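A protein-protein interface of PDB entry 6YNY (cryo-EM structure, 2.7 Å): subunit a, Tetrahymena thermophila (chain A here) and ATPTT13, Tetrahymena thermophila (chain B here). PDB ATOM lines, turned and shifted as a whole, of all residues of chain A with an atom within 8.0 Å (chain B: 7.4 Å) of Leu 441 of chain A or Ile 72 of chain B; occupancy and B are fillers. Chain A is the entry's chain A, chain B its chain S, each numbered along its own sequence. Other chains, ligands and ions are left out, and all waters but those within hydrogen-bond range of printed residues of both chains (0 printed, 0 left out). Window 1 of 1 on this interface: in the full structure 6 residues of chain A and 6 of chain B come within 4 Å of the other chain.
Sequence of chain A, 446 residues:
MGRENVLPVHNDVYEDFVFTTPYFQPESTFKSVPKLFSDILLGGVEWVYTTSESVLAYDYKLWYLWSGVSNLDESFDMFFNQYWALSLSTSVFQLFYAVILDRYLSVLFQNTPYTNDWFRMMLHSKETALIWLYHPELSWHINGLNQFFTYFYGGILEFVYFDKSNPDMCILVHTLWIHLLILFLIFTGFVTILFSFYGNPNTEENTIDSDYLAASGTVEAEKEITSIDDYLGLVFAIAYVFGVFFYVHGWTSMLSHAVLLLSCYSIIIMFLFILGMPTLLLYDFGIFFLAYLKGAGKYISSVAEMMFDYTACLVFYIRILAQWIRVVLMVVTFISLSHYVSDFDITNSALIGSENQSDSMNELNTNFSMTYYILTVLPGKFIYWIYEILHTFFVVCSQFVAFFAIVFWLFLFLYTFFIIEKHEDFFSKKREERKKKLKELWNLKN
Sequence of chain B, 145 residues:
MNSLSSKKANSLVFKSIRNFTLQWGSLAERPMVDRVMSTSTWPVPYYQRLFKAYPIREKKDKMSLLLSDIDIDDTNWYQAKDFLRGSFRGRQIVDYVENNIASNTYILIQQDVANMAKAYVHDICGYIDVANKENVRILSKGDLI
The backbone carbonyl oxygen (O) of Leu 441 of chain A lies within hydrogen-bond range of the backbone NH (N) of Asn 446 of chain A (3.3 Å).
Of the printed residues of chain B, Glu 440 of chain A touches Ile 109. Of the printed residues of chain B, Leu 441 of chain A touches Ile 72. Of the printed residues of chain B, Leu 444 of chain A touches Ile 109. Of the printed residues of chain B, Asn 446 of chain A touches Asp 71. Printed residues of chain A within 4 Å of Asp 71 of chain B: Asn 446 (2.7 Å). Ile 72 of chain B touches one residue of chain A. Printed residues of chain A within 4 Å of Ile 109 of chain B: Glu 440 (3.8 Å) and Leu 444 (3.7 Å). The nearest residue of chain B that does not touch Leu 441 of chain A is Ile 109 of chain B (4.1 Å). The nearest residue of chain A that does not touch Ile 72 of chain B is Leu 444 of chain A (5.8 Å). The nearest printed residue of chain B that does not touch Asn 446 of chain A is Ile 72 of chain B (6.2 Å).
Along chain A the printed residues that touch a printed residue of chain B span positions 440 to 446.
Among the printed residues, merely in contact across the chains: Leu 444 of chain A with Ile 109 of chain B (3.7 Å), Glu 440 of chain A with Ile 109 of chain B (3.8 Å) and Leu 441 of chain A with Ile 72 of chain B (3.9 Å).
O of Asn 446 of chain A lies close to OD2 of Asp 71 of chain B, at 2.7 Å.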
ATOM      1  N   LYS A 435     -16.017 -19.692 -26.576  1.00  0.00           N
ATOM      2  CA  LYS A 435     -17.465 -19.627 -26.433  1.00  0.00           C
ATOM      3  C   LYS A 435     -18.157 -20.708 -27.249  1.00  0.00           C
ATOM      4  O   LYS A 435     -19.244 -21.163 -26.876  1.00  0.00           O
ATOM      5  CB  LYS A 435     -17.974 -18.248 -26.844  1.00  0.00           C
ATOM      6  CG  LYS A 435     -19.454 -18.056 -26.600  1.00  0.00           C
ATOM      7  CD  LYS A 435     -19.910 -16.659 -26.971  1.00  0.00           C
ATOM      8  CE  LYS A 435     -21.421 -16.524 -26.854  1.00  0.00           C
ATOM      9  NZ  LYS A 435     -21.919 -16.880 -25.495  1.00  0.00           N
ATOM     10  N   LYS A 436     -17.557 -21.123 -28.365  1.00  0.00           N
ATOM     11  CA  LYS A 436     -18.123 -22.221 -29.138  1.00  0.00           C
ATOM     12  C   LYS A 436     -17.902 -23.556 -28.444  1.00  0.00           C
ATOM     13  O   LYS A 436     -18.690 -24.489 -28.628  1.00  0.00           O
ATOM     14  CB  LYS A 436     -17.515 -22.245 -30.536  1.00  0.00           C
ATOM     15  CG  LYS A 436     -17.731 -20.966 -31.321  1.00  0.00           C
ATOM     16  CD  LYS A 436     -16.966 -20.970 -32.635  1.00  0.00           C
ATOM     17  CE  LYS A 436     -17.505 -22.006 -33.605  1.00  0.00           C
ATOM     18  NZ  LYS A 436     -18.925 -21.746 -33.968  1.00  0.00           N
ATOM     19  N   LYS A 437     -16.838 -23.663 -27.649  1.00  0.00           N
ATOM     20  CA  LYS A 437     -16.593 -24.885 -26.893  1.00  0.00           C
ATOM     21  C   LYS A 437     -17.608 -25.057 -25.770  1.00  0.00           C
ATOM     22  O   LYS A 437     -17.879 -26.186 -25.349  1.00  0.00           O
ATOM     23  CB  LYS A 437     -15.166 -24.860 -26.346  1.00  0.00           C
ATOM     24  CG  LYS A 437     -14.749 -26.088 -25.558  1.00  0.00           C
ATOM     25  CD  LYS A 437     -14.705 -27.327 -26.431  1.00  0.00           C
ATOM     26  CE  LYS A 437     -14.251 -28.541 -25.645  1.00  0.00           C
ATOM     27  NZ  LYS A 437     -14.133 -29.743 -26.509  1.00  0.00           N
ATOM     28  N   LEU A 438     -18.177 -23.956 -25.277  1.00  0.00           N
ATOM     29  CA  LEU A 438     -19.185 -23.972 -24.226  1.00  0.00           C
ATOM     30  C   LEU A 438     -20.588 -23.712 -24.759  1.00  0.00           C
ATOM     31  O   LEU A 438     -21.463 -23.282 -24.002  1.00  0.00           O
ATOM     32  CB  LEU A 438     -18.838 -22.936 -23.158  1.00  0.00           C
ATOM     33  CG  LEU A 438     -17.753 -23.273 -22.137  1.00  0.00           C
ATOM     34  CD1 LEU A 438     -16.508 -23.800 -22.807  1.00  0.00           C
ATOM     35  CD2 LEU A 438     -17.429 -22.026 -21.344  1.00  0.00           C
ATOM     36  N   LYS A 439     -20.822 -23.967 -26.045  1.00  0.00           N
ATOM     37  CA  LYS A 439     -22.116 -23.649 -26.637  1.00  0.00           C
ATOM     38  C   LYS A 439     -23.233 -24.486 -26.027  1.00  0.00           C
ATOM     39  O   LYS A 439     -24.354 -24.000 -25.845  1.00  0.00           O
ATOM     40  CB  LYS A 439     -22.055 -23.864 -28.146  1.00  0.00           C
ATOM     41  CG  LYS A 439     -23.304 -23.452 -28.889  1.00  0.00           C
ATOM     42  CD  LYS A 439     -23.193 -23.783 -30.363  1.00  0.00           C
ATOM     43  CE  LYS A 439     -24.427 -23.344 -31.126  1.00  0.00           C
ATOM     44  NZ  LYS A 439     -25.660 -24.002 -30.620  1.00  0.00           N
ATOM     45  N   GLU A 440     -22.947 -25.746 -25.706  1.00  0.00           N
ATOM     46  CA  GLU A 440     -23.989 -26.627 -25.194  1.00  0.00           C
ATOM     47  C   GLU A 440     -24.364 -26.273 -23.763  1.00  0.00           C
ATOM     48  O   GLU A 440     -25.545 -26.296 -23.402  1.00  0.00           O
ATOM     49  CB  GLU A 440     -23.535 -28.081 -25.280  1.00  0.00           C
ATOM     50  CG  GLU A 440     -23.289 -28.573 -26.696  1.00  0.00           C
ATOM     51  CD  GLU A 440     -21.976 -28.078 -27.273  1.00  0.00           C
ATOM     52  OE1 GLU A 440     -21.231 -27.384 -26.549  1.00  0.00           O
ATOM     53  OE2 GLU A 440     -21.691 -28.379 -28.451  1.00  0.00           O
ATOM     54  N   LEU A 441     -23.374 -25.942 -22.935  1.00  0.00           N
ATOM     55  CA  LEU A 441     -23.667 -25.576 -21.555  1.00  0.00           C
ATOM     56  C   LEU A 441     -24.513 -24.313 -21.489  1.00  0.00           C
ATOM     57  O   LEU A 441     -25.409 -24.201 -20.644  1.00  0.00           O
ATOM     58  CB  LEU A 441     -22.366 -25.398 -20.778  1.00  0.00           C
ATOM     59  CG  LEU A 441     -22.504 -24.900 -19.340  1.00  0.00           C
ATOM     60  CD1 LEU A 441     -23.478 -25.751 -18.550  1.00  0.00           C
ATOM     61  CD2 LEU A 441     -21.149 -24.892 -18.678  1.00  0.00           C
ATOM     62  N   TRP A 442     -24.244 -23.347 -22.368  1.00  0.00           N
ATOM     63  CA  TRP A 442     -25.095 -22.164 -22.430  1.00  0.00           C
ATOM     64  C   TRP A 442     -26.504 -22.523 -22.875  1.00  0.00           C
ATOM     65  O   TRP A 442     -27.481 -21.928 -22.407  1.00  0.00           O
ATOM     66  CB  TRP A 442     -24.493 -21.129 -23.374  1.00  0.00           C
ATOM     67  CG  TRP A 442     -23.392 -20.333 -22.772  1.00  0.00           C
ATOM     68  CD1 TRP A 442     -22.067 -20.410 -23.072  1.00  0.00           C
ATOM     69  CD2 TRP A 442     -23.517 -19.332 -21.760  1.00  0.00           C
ATOM     70  NE1 TRP A 442     -21.358 -19.516 -22.311  1.00  0.00           N
ATOM     71  CE2 TRP A 442     -22.227 -18.843 -21.495  1.00  0.00           C
ATOM     72  CE3 TRP A 442     -24.596 -18.803 -21.050  1.00  0.00           C
ATOM     73  CZ2 TRP A 442     -21.986 -17.851 -20.553  1.00  0.00           C
ATOM     74  CZ3 TRP A 442     -24.356 -17.820 -20.116  1.00  0.00           C
ATOM     75  CH2 TRP A 442     -23.060 -17.353 -19.876  1.00  0.00           C
ATOM     76  N   ASN A 443     -26.633 -23.495 -23.781  1.00  0.00           N
ATOM     77  CA  ASN A 443     -27.955 -23.910 -24.229  1.00  0.00           C
ATOM     78  C   ASN A 443     -28.807 -24.389 -23.064  1.00  0.00           C
ATOM     79  O   ASN A 443     -30.034 -24.242 -23.089  1.00  0.00           O
ATOM     80  CB  ASN A 443     -27.823 -25.005 -25.285  1.00  0.00           C
ATOM     81  CG  ASN A 443     -29.141 -25.341 -25.944  1.00  0.00           C
ATOM     82  OD1 ASN A 443     -29.905 -26.169 -25.451  1.00  0.00           O
ATOM     83  ND2 ASN A 443     -29.414 -24.698 -27.071  1.00  0.00           N
ATOM     84  N   LEU A 444     -28.179 -24.956 -22.040  1.00  0.00           N
ATOM     85  CA  LEU A 444     -28.877 -25.352 -20.825  1.00  0.00           C
ATOM     86  C   LEU A 444     -29.176 -24.174 -19.912  1.00  0.00           C
ATOM     87  O   LEU A 444     -29.741 -24.378 -18.833  1.00  0.00           O
ATOM     88  CB  LEU A 444     -28.053 -26.384 -20.059  1.00  0.00           C
ATOM     89  CG  LEU A 444     -27.564 -27.593 -20.848  1.00  0.00           C
ATOM     90  CD1 LEU A 444     -26.696 -28.462 -19.973  1.00  0.00           C
ATOM     91  CD2 LEU A 444     -28.729 -28.384 -21.389  1.00  0.00           C
ATOM     92  N   LYS A 445     -28.812 -22.957 -20.314  1.00  0.00           N
ATOM     93  CA  LYS A 445     -28.998 -21.767 -19.489  1.00  0.00           C
ATOM     94  C   LYS A 445     -28.180 -21.847 -18.209  1.00  0.00           C
ATOM     95  O   LYS A 445     -28.605 -21.365 -17.156  1.00  0.00           O
ATOM     96  CB  LYS A 445     -30.476 -21.540 -19.172  1.00  0.00           C
ATOM     97  CG  LYS A 445     -31.339 -21.408 -20.409  1.00  0.00           C
ATOM     98  CD  LYS A 445     -32.779 -21.110 -20.054  1.00  0.00           C
ATOM     99  CE  LYS A 445     -33.638 -21.032 -21.297  1.00  0.00           C
ATOM    100  NZ  LYS A 445     -33.153 -19.985 -22.240  1.00  0.00           N
ATOM    101  N   ASN A 446     -27.000 -22.452 -18.304  1.00  0.00           N
ATOM    102  CA  ASN A 446     -26.085 -22.608 -17.178  1.00  0.00           C
ATOM    103  C   ASN A 446     -26.814 -22.998 -15.897  1.00  0.00           C
ATOM    104  O   ASN A 446     -26.546 -24.049 -15.317  1.00  0.00           O
ATOM    105  CB  ASN A 446     -25.293 -21.320 -16.956  1.00  0.00           C
ATOM    106  CG  ASN A 446     -26.125 -20.225 -16.339  1.00  0.00           C
ATOM    107  OD1 ASN A 446     -26.744 -19.427 -17.041  1.00  0.00           O
ATOM    108  ND2 ASN A 446     -26.148 -20.181 -15.013  1.00  0.00           N
ATOM    109  N   ASP B  69     -22.585 -23.427  -6.172  1.00  0.00           N
ATOM    110  CA  ASP B  69     -23.363 -23.223  -7.391  1.00  0.00           C
ATOM    111  C   ASP B  69     -22.452 -23.182  -8.602  1.00  0.00           C
ATOM    112  O   ASP B  69     -22.556 -22.309  -9.466  1.00  0.00           O
ATOM    113  CB  ASP B  69     -24.187 -21.944  -7.303  1.00  0.00           C
ATOM    114  CG  ASP B  69     -23.337 -20.717  -7.058  1.00  0.00           C
ATOM    115  OD1 ASP B  69     -22.313 -20.833  -6.357  1.00  0.00           O
ATOM    116  OD2 ASP B  69     -23.696 -19.633  -7.564  1.00  0.00           O
ATOM    117  N   ILE B  70     -21.541 -24.138  -8.677  1.00  0.00           N
ATOM    118  CA  ILE B  70     -20.585 -24.215  -9.771  1.00  0.00           C
ATOM    119  C   ILE B  70     -21.159 -25.118 -10.850  1.00  0.00           C
ATOM    120  O   ILE B  70     -21.540 -26.262 -10.581  1.00  0.00           O
ATOM    121  CB  ILE B  70     -19.227 -24.732  -9.274  1.00  0.00           C
ATOM    122  CG1 ILE B  70     -18.696 -23.822  -8.167  1.00  0.00           C
ATOM    123  CG2 ILE B  70     -18.240 -24.786 -10.412  1.00  0.00           C
ATOM    124  CD1 ILE B  70     -17.563 -24.409  -7.381  1.00  0.00           C
ATOM    125  N   ASP B  71     -21.229 -24.601 -12.072  1.00  0.00           N
ATOM    126  CA  ASP B  71     -21.794 -25.358 -13.173  1.00  0.00           C
ATOM    127  C   ASP B  71     -20.915 -26.560 -13.506  1.00  0.00           C
ATOM    128  O   ASP B  71     -19.795 -26.712 -13.011  1.00  0.00           O
ATOM    129  CB  ASP B  71     -21.960 -24.467 -14.399  1.00  0.00           C
ATOM    130  CG  ASP B  71     -22.948 -23.343 -14.174  1.00  0.00           C
ATOM    131  OD1 ASP B  71     -22.661 -22.450 -13.350  1.00  0.00           O
ATOM    132  OD2 ASP B  71     -24.013 -23.352 -14.823  1.00  0.00           O
ATOM    133  N   ILE B  72     -21.449 -27.426 -14.367  1.00  0.00           N
ATOM    134  CA  ILE B  72     -20.729 -28.622 -14.778  1.00  0.00           C
ATOM    135  C   ILE B  72     -19.404 -28.234 -15.414  1.00  0.00           C
ATOM    136  O   ILE B  72     -19.318 -27.263 -16.176  1.00  0.00           O
ATOM    137  CB  ILE B  72     -21.602 -29.446 -15.740  1.00  0.00           C
ATOM    138  CG1 ILE B  72     -21.102 -30.881 -15.827  1.00  0.00           C
ATOM    139  CG2 ILE B  72     -21.628 -28.819 -17.112  1.00  0.00           C
ATOM    140  CD1 ILE B  72     -21.542 -31.720 -14.680  1.00  0.00           C
ATOM    141  N   ASP B  73     -18.357 -28.992 -15.101  1.00  0.00           N
ATOM    142  CA  ASP B  73     -17.027 -28.708 -15.618  1.00  0.00           C
ATOM    143  C   ASP B  73     -16.238 -30.009 -15.685  1.00  0.00           C
ATOM    144  O   ASP B  73     -16.789 -31.101 -15.524  1.00  0.00           O
ATOM    145  CB  ASP B  73     -16.319 -27.652 -14.759  1.00  0.00           C
ATOM    146  CG  ASP B  73     -16.066 -28.122 -13.341  1.00  0.00           C
ATOM    147  OD1 ASP B  73     -16.547 -29.211 -12.972  1.00  0.00           O
ATOM    148  OD2 ASP B  73     -15.377 -27.398 -12.594  1.00  0.00           O
ATOM    149  N   ASP B  74     -14.932 -29.884 -15.924  1.00  0.00           N
ATOM    150  CA  ASP B  74     -14.091 -31.060 -16.106  1.00  0.00           C
ATOM    151  C   ASP B  74     -13.934 -31.854 -14.818  1.00  0.00           C
ATOM    152  O   ASP B  74     -13.707 -33.067 -14.864  1.00  0.00           O
ATOM    153  CB  ASP B  74     -12.718 -30.645 -16.629  1.00  0.00           C
ATOM    154  CG  ASP B  74     -12.778 -30.048 -18.017  1.00  0.00           C
ATOM    155  OD1 ASP B  74     -13.553 -30.554 -18.852  1.00  0.00           O
ATOM    156  OD2 ASP B  74     -12.047 -29.070 -18.272  1.00  0.00           O
ATOM    157  N   THR B  75     -14.046 -31.196 -13.666  1.00  0.00           N
ATOM    158  CA  THR B  75     -13.866 -31.888 -12.400  1.00  0.00           C
ATOM    159  C   THR B  75     -14.949 -32.925 -12.150  1.00  0.00           C
ATOM    160  O   THR B  75     -14.766 -33.803 -11.303  1.00  0.00           O
ATOM    161  CB  THR B  75     -13.844 -30.885 -11.249  1.00  0.00           C
ATOM    162  OG1 THR B  75     -15.003 -30.049 -11.316  1.00  0.00           O
ATOM    163  CG2 THR B  75     -12.601 -30.029 -11.311  1.00  0.00           C
ATOM    164  N   ASN B  76     -16.067 -32.848 -12.868  1.00  0.00           N
ATOM    165  CA  ASN B  76     -17.154 -33.791 -12.651  1.00  0.00           C
ATOM    166  C   ASN B  76     -16.837 -35.151 -13.254  1.00  0.00           C
ATOM    167  O   ASN B  76     -17.083 -36.182 -12.620  1.00  0.00           O
ATOM    168  CB  ASN B  76     -18.448 -33.237 -13.236  1.00  0.00           C
ATOM    169  CG  ASN B  76     -18.859 -31.930 -12.602  1.00  0.00           C
ATOM    170  OD1 ASN B  76     -18.578 -30.856 -13.125  1.00  0.00           O
ATOM    171  ND2 ASN B  76     -19.527 -32.016 -11.466  1.00  0.00           N
ATOM    172  N   TRP B  77     -16.297 -35.179 -14.472  1.00  0.00           N
ATOM    173  CA  TRP B  77     -15.972 -36.454 -15.090  1.00  0.00           C
ATOM    174  C   TRP B  77     -14.660 -37.023 -14.572  1.00  0.00           C
ATOM    175  O   TRP B  77     -14.476 -38.244 -14.585  1.00  0.00           O
ATOM    176  CB  TRP B  77     -15.928 -36.321 -16.614  1.00  0.00           C
ATOM    177  CG  TRP B  77     -14.880 -35.416 -17.162  1.00  0.00           C
ATOM    178  CD1 TRP B  77     -15.058 -34.151 -17.622  1.00  0.00           C
ATOM    179  CD2 TRP B  77     -13.492 -35.713 -17.334  1.00  0.00           C
ATOM    180  NE1 TRP B  77     -13.869 -33.635 -18.065  1.00  0.00           N
ATOM    181  CE2 TRP B  77     -12.890 -34.576 -17.896  1.00  0.00           C
ATOM    182  CE3 TRP B  77     -12.699 -36.828 -17.063  1.00  0.00           C
ATOM    183  CZ2 TRP B  77     -11.536 -34.520 -18.191  1.00  0.00           C
ATOM    184  CZ3 TRP B  77     -11.357 -36.770 -17.355  1.00  0.00           C
ATOM    185  CH2 TRP B  77     -10.788 -35.626 -17.912  1.00  0.00           C
ATOM    186  N   ILE B 107     -17.386 -33.963 -21.175  1.00  0.00           N
ATOM    187  CA  ILE B 107     -18.548 -33.318 -20.570  1.00  0.00           C
ATOM    188  C   ILE B 107     -19.726 -33.665 -21.470  1.00  0.00           C
ATOM    189  O   ILE B 107     -20.105 -32.913 -22.366  1.00  0.00           O
ATOM    190  CB  ILE B 107     -18.355 -31.813 -20.416  1.00  0.00           C
ATOM    191  CG1 ILE B 107     -17.031 -31.518 -19.713  1.00  0.00           C
ATOM    192  CG2 ILE B 107     -19.511 -31.220 -19.637  1.00  0.00           C
ATOM    193  CD1 ILE B 107     -16.734 -30.055 -19.557  1.00  0.00           C
ATOM    194  N   LEU B 108     -20.310 -34.830 -21.220  1.00  0.00           N
ATOM    195  CA  LEU B 108     -21.394 -35.333 -22.044  1.00  0.00           C
ATOM    196  C   LEU B 108     -22.692 -34.627 -21.689  1.00  0.00           C
ATOM    197  O   LEU B 108     -23.085 -34.575 -20.520  1.00  0.00           O
ATOM    198  CB  LEU B 108     -21.534 -36.840 -21.861  1.00  0.00           C
ATOM    199  CG  LEU B 108     -20.258 -37.622 -22.156  1.00  0.00           C
ATOM    200  CD1 LEU B 108     -20.491 -39.100 -21.983  1.00  0.00           C
ATOM    201  CD2 LEU B 108     -19.771 -37.322 -23.550  1.00  0.00           C
ATOM    202  N   ILE B 109     -23.355 -34.083 -22.703  1.00  0.00           N
ATOM    203  CA  ILE B 109     -24.604 -33.359 -22.537  1.00  0.00           C
ATOM    204  C   ILE B 109     -25.591 -33.915 -23.549  1.00  0.00           C
ATOM    205  O   ILE B 109     -25.372 -33.802 -24.761  1.00  0.00           O
ATOM    206  CB  ILE B 109     -24.425 -31.846 -22.729  1.00  0.00           C
ATOM    207  CG1 ILE B 109     -23.303 -31.335 -21.829  1.00  0.00           C
ATOM    208  CG2 ILE B 109     -25.708 -31.122 -22.408  1.00  0.00           C
ATOM    209  CD1 ILE B 109     -23.035 -29.864 -21.959  1.00  0.00           C
